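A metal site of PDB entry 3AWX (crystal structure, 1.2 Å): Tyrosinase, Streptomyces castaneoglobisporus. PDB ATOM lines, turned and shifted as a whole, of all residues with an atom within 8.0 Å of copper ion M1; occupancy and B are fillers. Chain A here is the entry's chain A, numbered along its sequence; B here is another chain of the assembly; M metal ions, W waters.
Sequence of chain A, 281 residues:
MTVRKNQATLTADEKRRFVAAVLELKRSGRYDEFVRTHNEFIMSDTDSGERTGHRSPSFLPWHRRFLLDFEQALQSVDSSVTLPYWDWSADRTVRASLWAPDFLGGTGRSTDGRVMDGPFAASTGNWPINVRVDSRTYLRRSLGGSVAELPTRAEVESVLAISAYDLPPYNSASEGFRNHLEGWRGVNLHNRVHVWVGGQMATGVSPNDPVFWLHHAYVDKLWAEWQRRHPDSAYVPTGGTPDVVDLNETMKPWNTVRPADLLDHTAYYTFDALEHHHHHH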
ATOM      1  N   HIS A  38      -7.907  -0.185   7.435  1.00  0.00           N
ATOM      2  CA  HIS A  38      -9.171  -0.317   6.705  1.00  0.00           C
ATOM      3  C   HIS A  38      -8.973  -0.405   5.201  1.00  0.00           C
ATOM      4  O   HIS A  38      -9.566  -1.239   4.510  1.00  0.00           O
ATOM      5  CB  HIS A  38     -10.073   0.890   7.041  1.00  0.00           C
ATOM      6  CG  HIS A  38     -11.436   0.692   6.396  1.00  0.00           C
ATOM      7  ND1 HIS A  38     -11.767   1.264   5.179  1.00  0.00           N
ATOM      8  CD2 HIS A  38     -12.543  -0.017   6.768  1.00  0.00           C
ATOM      9  CE1 HIS A  38     -13.019   0.907   4.866  1.00  0.00           C
ATOM     10  NE2 HIS A  38     -13.531   0.130   5.827  1.00  0.00           N
ATOM     11  N   ILE A  42     -10.167  -3.350   2.639  1.00  0.00           N
ATOM     12  CA  ILE A  42     -11.224  -3.154   1.645  1.00  0.00           C
ATOM     13  C   ILE A  42     -10.668  -3.370   0.256  1.00  0.00           C
ATOM     14  O   ILE A  42     -11.375  -3.768  -0.680  1.00  0.00           O
ATOM     15  CB  ILE A  42     -11.886  -1.774   1.832  1.00  0.00           C
ATOM     16  CG1 ILE A  42     -13.287  -1.777   1.188  1.00  0.00           C
ATOM     17  CG2 ILE A  42     -11.000  -0.656   1.366  1.00  0.00           C
ATOM     18  CD1 ILE A  42     -14.029  -0.467   1.390  1.00  0.00           C
ATOM     19  N   GLY A  53     -13.225  -8.276   5.790  1.00  0.00           N
ATOM     20  CA  GLY A  53     -13.806  -7.070   6.370  1.00  0.00           C
ATOM     21  C   GLY A  53     -15.094  -6.608   5.722  1.00  0.00           C
ATOM     22  O   GLY A  53     -15.895  -5.885   6.301  1.00  0.00           O
ATOM     23  N   HIS A  54     -15.292  -6.969   4.458  1.00  0.00           N
ATOM     24  CA  HIS A  54     -16.332  -6.475   3.591  1.00  0.00           C
ATOM     25  C   HIS A  54     -16.878  -7.617   2.739  1.00  0.00           C
ATOM     26  O   HIS A  54     -16.247  -8.649   2.543  1.00  0.00           O
ATOM     27  CB  HIS A  54     -15.769  -5.367   2.637  1.00  0.00           C
ATOM     28  CG  HIS A  54     -15.172  -4.236   3.460  1.00  0.00           C
ATOM     29  ND1 HIS A  54     -13.884  -4.239   3.928  1.00  0.00           N
ATOM     30  CD2 HIS A  54     -15.764  -3.085   3.923  1.00  0.00           C
ATOM     31  CE1 HIS A  54     -13.735  -3.124   4.670  1.00  0.00           C
ATOM     32  NE2 HIS A  54     -14.866  -2.387   4.667  1.00  0.00           N
ATOM     33  N   PHE A  59     -18.259  -8.999   7.664  1.00  0.00           N
ATOM     34  CA  PHE A  59     -18.346  -7.539   7.604  1.00  0.00           C
ATOM     35  C   PHE A  59     -18.773  -6.953   8.969  1.00  0.00           C
ATOM     36  O   PHE A  59     -18.162  -5.964   9.444  1.00  0.00           O
ATOM     37  CB  PHE A  59     -19.376  -7.169   6.558  1.00  0.00           C
ATOM     38  CG  PHE A  59     -19.871  -5.691   6.568  1.00  0.00           C
ATOM     39  CD1 PHE A  59     -19.023  -4.651   6.224  1.00  0.00           C
ATOM     40  CD2 PHE A  59     -21.192  -5.437   6.898  1.00  0.00           C
ATOM     41  CE1 PHE A  59     -19.480  -3.342   6.238  1.00  0.00           C
ATOM     42  CE2 PHE A  59     -21.648  -4.098   6.903  1.00  0.00           C
ATOM     43  CZ  PHE A  59     -20.802  -3.074   6.552  1.00  0.00           C
ATOM     44  N   HIS A  63     -16.051  -5.058  11.516  1.00  0.00           N
ATOM     45  CA  HIS A  63     -16.147  -3.631  11.863  1.00  0.00           C
ATOM     46  C   HIS A  63     -16.446  -3.446  13.340  1.00  0.00           C
ATOM     47  O   HIS A  63     -16.038  -2.452  13.940  1.00  0.00           O
ATOM     48  CB  HIS A  63     -17.201  -2.932  10.983  1.00  0.00           C
ATOM     49  CG  HIS A  63     -16.677  -2.673   9.592  1.00  0.00           C
ATOM     50  ND1 HIS A  63     -16.677  -3.652   8.594  1.00  0.00           N
ATOM     51  CD2 HIS A  63     -16.066  -1.578   9.056  1.00  0.00           C
ATOM     52  CE1 HIS A  63     -16.119  -3.174   7.493  1.00  0.00           C
ATOM     53  NE2 HIS A  63     -15.757  -1.904   7.735  1.00  0.00           N
ATOM     54  N   GLU A 182     -25.230  -4.109   4.549  1.00  0.00           N
ATOM     55  CA  GLU A 182     -23.995  -3.595   3.895  1.00  0.00           C
ATOM     56  C   GLU A 182     -24.354  -2.738   2.702  1.00  0.00           C
ATOM     57  O   GLU A 182     -23.838  -1.635   2.537  1.00  0.00           O
ATOM     58  CB  GLU A 182     -23.080  -4.777   3.557  1.00  0.00           C
ATOM     59  CG  GLU A 182     -21.696  -4.290   3.110  1.00  0.00           C
ATOM     60  CD  GLU A 182     -20.708  -5.393   2.881  1.00  0.00           C
ATOM     61  OE1 GLU A 182     -21.031  -6.566   3.159  1.00  0.00           O
ATOM     62  OE2 GLU A 182     -19.590  -5.059   2.421  1.00  0.00           O
ATOM     63  N   HIS A 190     -25.761   0.784   4.288  1.00  0.00           N
ATOM     64  CA  HIS A 190     -24.442   1.286   4.684  1.00  0.00           C
ATOM     65  C   HIS A 190     -23.637   1.851   3.537  1.00  0.00           C
ATOM     66  O   HIS A 190     -22.981   2.891   3.702  1.00  0.00           O
ATOM     67  CB  HIS A 190     -23.663   0.090   5.338  1.00  0.00           C
ATOM     68  CG  HIS A 190     -22.176   0.132   5.145  1.00  0.00           C
ATOM     69  ND1 HIS A 190     -21.580  -0.385   4.014  1.00  0.00           N
ATOM     70  CD2 HIS A 190     -21.177   0.621   5.892  1.00  0.00           C
ATOM     71  CE1 HIS A 190     -20.264  -0.205   4.098  1.00  0.00           C
ATOM     72  NE2 HIS A 190     -19.964   0.424   5.250  1.00  0.00           N
ATOM     73  N   ASN A 191     -23.684   1.212   2.346  1.00  0.00           N
ATOM     74  CA  ASN A 191     -22.855   1.766   1.238  1.00  0.00           C
ATOM     75  C   ASN A 191     -23.360   3.128   0.821  1.00  0.00           C
ATOM     76  O   ASN A 191     -22.580   4.047   0.573  1.00  0.00           O
ATOM     77  CB  ASN A 191     -22.866   0.846   0.027  1.00  0.00           C
ATOM     78  CG  ASN A 191     -22.037  -0.405   0.183  1.00  0.00           C
ATOM     79  OD1 ASN A 191     -21.293  -0.602   1.151  1.00  0.00           O
ATOM     80  ND2 ASN A 191     -22.200  -1.302  -0.788  1.00  0.00           N
ATOM     81  N   VAL A 193     -24.782   5.446   2.590  1.00  0.00           N
ATOM     82  CA  VAL A 193     -24.349   6.527   3.471  1.00  0.00           C
ATOM     83  C   VAL A 193     -22.917   6.979   3.143  1.00  0.00           C
ATOM     84  O   VAL A 193     -22.642   8.187   3.121  1.00  0.00           O
ATOM     85  CB  VAL A 193     -24.466   6.089   4.936  1.00  0.00           C
ATOM     86  CG1 VAL A 193     -23.882   7.182   5.859  1.00  0.00           C
ATOM     87  CG2 VAL A 193     -25.926   5.747   5.297  1.00  0.00           C
ATOM     88  N   HIS A 194     -21.999   6.012   2.856  1.00  0.00           N
ATOM     89  CA  HIS A 194     -20.676   6.442   2.418  1.00  0.00           C
ATOM     90  C   HIS A 194     -20.742   7.332   1.183  1.00  0.00           C
ATOM     91  O   HIS A 194     -20.043   8.363   1.103  1.00  0.00           O
ATOM     92  CB  HIS A 194     -19.827   5.225   2.138  1.00  0.00           C
ATOM     93  CG  HIS A 194     -19.204   4.486   3.270  1.00  0.00           C
ATOM     94  ND1 HIS A 194     -18.008   4.900   3.864  1.00  0.00           N
ATOM     95  CD2 HIS A 194     -19.527   3.330   3.909  1.00  0.00           C
ATOM     96  CE1 HIS A 194     -17.672   4.004   4.810  1.00  0.00           C
ATOM     97  NE2 HIS A 194     -18.577   3.044   4.862  1.00  0.00           N
ATOM     98  N   MET A 201     -14.808   9.810   2.643  1.00  0.00           N
ATOM     99  CA  MET A 201     -15.748   8.809   3.149  1.00  0.00           C
ATOM    100  C   MET A 201     -16.277   7.910   2.077  1.00  0.00           C
ATOM    101  O   MET A 201     -16.813   6.829   2.354  1.00  0.00           O
ATOM    102  CB  MET A 201     -16.838   9.596   3.859  1.00  0.00           C
ATOM    103  CG  MET A 201     -17.841   8.772   4.618  1.00  0.00           C
ATOM    104  SD  MET A 201     -17.184   7.740   5.955  1.00  0.00           S
ATOM    105  CE  MET A 201     -18.810   7.155   6.445  1.00  0.00           C
ATOM    106  N   THR A 203     -14.373   6.582  -0.287  1.00  0.00           N
ATOM    107  CA  THR A 203     -13.198   5.857  -0.783  1.00  0.00           C
ATOM    108  C   THR A 203     -12.725   4.782   0.187  1.00  0.00           C
ATOM    109  O   THR A 203     -13.224   4.647   1.292  1.00  0.00           O
ATOM    110  CB  THR A 203     -12.012   6.800  -1.056  1.00  0.00           C
ATOM    111  OG1 THR A 203     -11.414   7.197   0.212  1.00  0.00           O
ATOM    112  CG2 THR A 203     -12.518   8.045  -1.779  1.00  0.00           C
ATOM    113  N   SER A 206     -11.809   5.749   3.789  1.00  0.00           N
ATOM    114  CA  SER A 206     -12.925   6.419   4.428  1.00  0.00           C
ATOM    115  C   SER A 206     -12.733   6.714   5.922  1.00  0.00           C
ATOM    116  O   SER A 206     -13.351   7.727   6.343  1.00  0.00           O
ATOM    117  CB  SER A 206     -14.186   5.593   4.153  1.00  0.00           C
ATOM    118  OG  SER A 206     -13.996   4.239   4.564  1.00  0.00           O
ATOM    119  N   PRO A 207     -11.952   5.999   6.719  1.00  0.00           N
ATOM    120  CA  PRO A 207     -11.739   6.477   8.108  1.00  0.00           C
ATOM    121  C   PRO A 207     -11.012   7.795   8.200  1.00  0.00           C
ATOM    122  O   PRO A 207     -10.920   8.329   9.307  1.00  0.00           O
ATOM    123  CB  PRO A 207     -10.960   5.314   8.787  1.00  0.00           C
ATOM    124  CG  PRO A 207     -11.306   4.119   7.929  1.00  0.00           C
ATOM    125  CD  PRO A 207     -11.334   4.658   6.543  1.00  0.00           C
ATOM    126  N   PHE A 212     -16.756   8.412   9.848  1.00  0.00           N
ATOM    127  CA  PHE A 212     -16.682   6.968   9.601  1.00  0.00           C
ATOM    128  C   PHE A 212     -17.119   6.173  10.830  1.00  0.00           C
ATOM    129  O   PHE A 212     -17.855   5.194  10.744  1.00  0.00           O
ATOM    130  CB  PHE A 212     -15.246   6.615   9.210  1.00  0.00           C
ATOM    131  CG  PHE A 212     -14.967   5.113   9.068  1.00  0.00           C
ATOM    132  CD1 PHE A 212     -14.648   4.295  10.145  1.00  0.00           C
ATOM    133  CD2 PHE A 212     -15.039   4.577   7.796  1.00  0.00           C
ATOM    134  CE1 PHE A 212     -14.437   2.953   9.998  1.00  0.00           C
ATOM    135  CE2 PHE A 212     -14.784   3.221   7.642  1.00  0.00           C
ATOM    136  CZ  PHE A 212     -14.500   2.397   8.726  1.00  0.00           C
ATOM    137  N   HIS A 215     -20.899   6.500  11.655  1.00  0.00           N
ATOM    138  CA  HIS A 215     -21.664   5.694  10.698  1.00  0.00           C
ATOM    139  C   HIS A 215     -21.575   4.241  11.121  1.00  0.00           C
ATOM    140  O   HIS A 215     -22.589   3.524  11.298  1.00  0.00           O
ATOM    141  CB  HIS A 215     -21.076   5.914   9.307  1.00  0.00           C
ATOM    142  CG  HIS A 215     -21.699   5.040   8.270  1.00  0.00           C
ATOM    143  ND1 HIS A 215     -23.037   4.680   8.349  1.00  0.00           N
ATOM    144  CD2 HIS A 215     -21.153   4.462   7.155  1.00  0.00           C
ATOM    145  CE1 HIS A 215     -23.278   3.929   7.267  1.00  0.00           C
ATOM    146  NE2 HIS A 215     -22.184   3.756   6.519  1.00  0.00           N
ATOM    147  N   HIS A 216     -20.330   3.738  11.253  1.00  0.00           N
ATOM    148  CA  HIS A 216     -20.226   2.298  11.597  1.00  0.00           C
ATOM    149  C   HIS A 216     -20.750   1.990  12.980  1.00  0.00           C
ATOM    150  O   HIS A 216     -21.184   0.848  13.213  1.00  0.00           O
ATOM    151  CB  HIS A 216     -18.775   1.811  11.399  1.00  0.00           C
ATOM    152  CG  HIS A 216     -18.635   1.344   9.961  1.00  0.00           C
ATOM    153  ND1 HIS A 216     -19.071   0.067   9.647  1.00  0.00           N
ATOM    154  CD2 HIS A 216     -18.203   1.914   8.811  1.00  0.00           C
ATOM    155  CE1 HIS A 216     -18.894  -0.113   8.326  1.00  0.00           C
ATOM    156  NE2 HIS A 216     -18.367   0.984   7.791  1.00  0.00           N
ATOM    157  N   VAL A 219     -24.386   1.353  12.137  1.00  0.00           N
ATOM    158  CA  VAL A 219     -24.483   0.048  11.472  1.00  0.00           C
ATOM    159  C   VAL A 219     -24.402  -1.080  12.495  1.00  0.00           C
ATOM    160  O   VAL A 219     -25.146  -2.039  12.433  1.00  0.00           O
ATOM    161  CB  VAL A 219     -23.384  -0.071  10.391  1.00  0.00           C
ATOM    162  CG1 VAL A 219     -23.308  -1.497   9.833  1.00  0.00           C
ATOM    163  CG2 VAL A 219     -23.633   0.932   9.258  1.00  0.00           C
ATOM    164  N   TYR B  98     -17.738   2.197  -2.677  1.00  0.00           N
ATOM    165  CA  TYR B  98     -19.051   1.789  -2.145  1.00  0.00           C
ATOM    166  C   TYR B  98     -20.152   2.020  -3.186  1.00  0.00           C
ATOM    167  O   TYR B  98     -21.343   2.033  -2.863  1.00  0.00           O
ATOM    168  CB  TYR B  98     -19.386   2.570  -0.876  1.00  0.00           C
ATOM    169  CG  TYR B  98     -18.317   2.460   0.227  1.00  0.00           C
ATOM    170  CD1 TYR B  98     -17.339   3.438   0.350  1.00  0.00           C
ATOM    171  CD2 TYR B  98     -18.285   1.406   1.118  1.00  0.00           C
ATOM    172  CE1 TYR B  98     -16.349   3.379   1.335  1.00  0.00           C
ATOM    173  CE2 TYR B  98     -17.321   1.306   2.126  1.00  0.00           C
ATOM    174  CZ  TYR B  98     -16.350   2.302   2.216  1.00  0.00           C
ATOM    175  OH  TYR B  98     -15.421   2.259   3.222  1.00  0.00           O
HETATM  176 CU    CU M   1     -18.200   1.186   5.674  1.00  0.00          CU
HETATM  177 CU    CU M   2     -15.466  -0.637   5.489  1.00  0.00          CU
HETATM  178  O   HOH W   1     -17.347  -0.757   5.154  1.00  0.00           O
HETATM  179  O   HOH W   2     -16.261   1.198   5.485  1.00  0.00           O
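Residues that only touch copper ion M1: Tyr 98 of chain B (3.7 Å).
Of the 20 residues printed, 4 come within 4 Å of copper ion M1.
The nearest printed residue that does not touch copper ion M1 is Phe 212 (4.4 Å).
ND1 of His 190 lies within hydrogen-bond range of OD1 of Asn 191, at 2.9 Å.
O of His 190 lies within hydrogen-bond range of NE2 of His 215 (3.1 Å).
A ring nitrogen (ND1) of His 194 lies within hydrogen-bond range of the backbone carbonyl oxygen of Met 201, at 2.7 Å.
A ring nitrogen (ND1) of His 190 lies within hydrogen-bond range of the backbone carbonyl oxygen (O) of Glu 182 (3.0 Å).
OH of Tyr 98 of chain B sits at hydrogen-bond distance from OG of Ser 206 (2.8 Å).
Copper ion M1 is bound by water W2 (1.9 Å), NE2 of His 190 (2.0 Å), NE2 of His 194 (2.1 Å), NE2 of His 216 (2.1 Å) and water W1 (2.2 Å).
Copper ion M1 has five donor atoms within binding distance.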
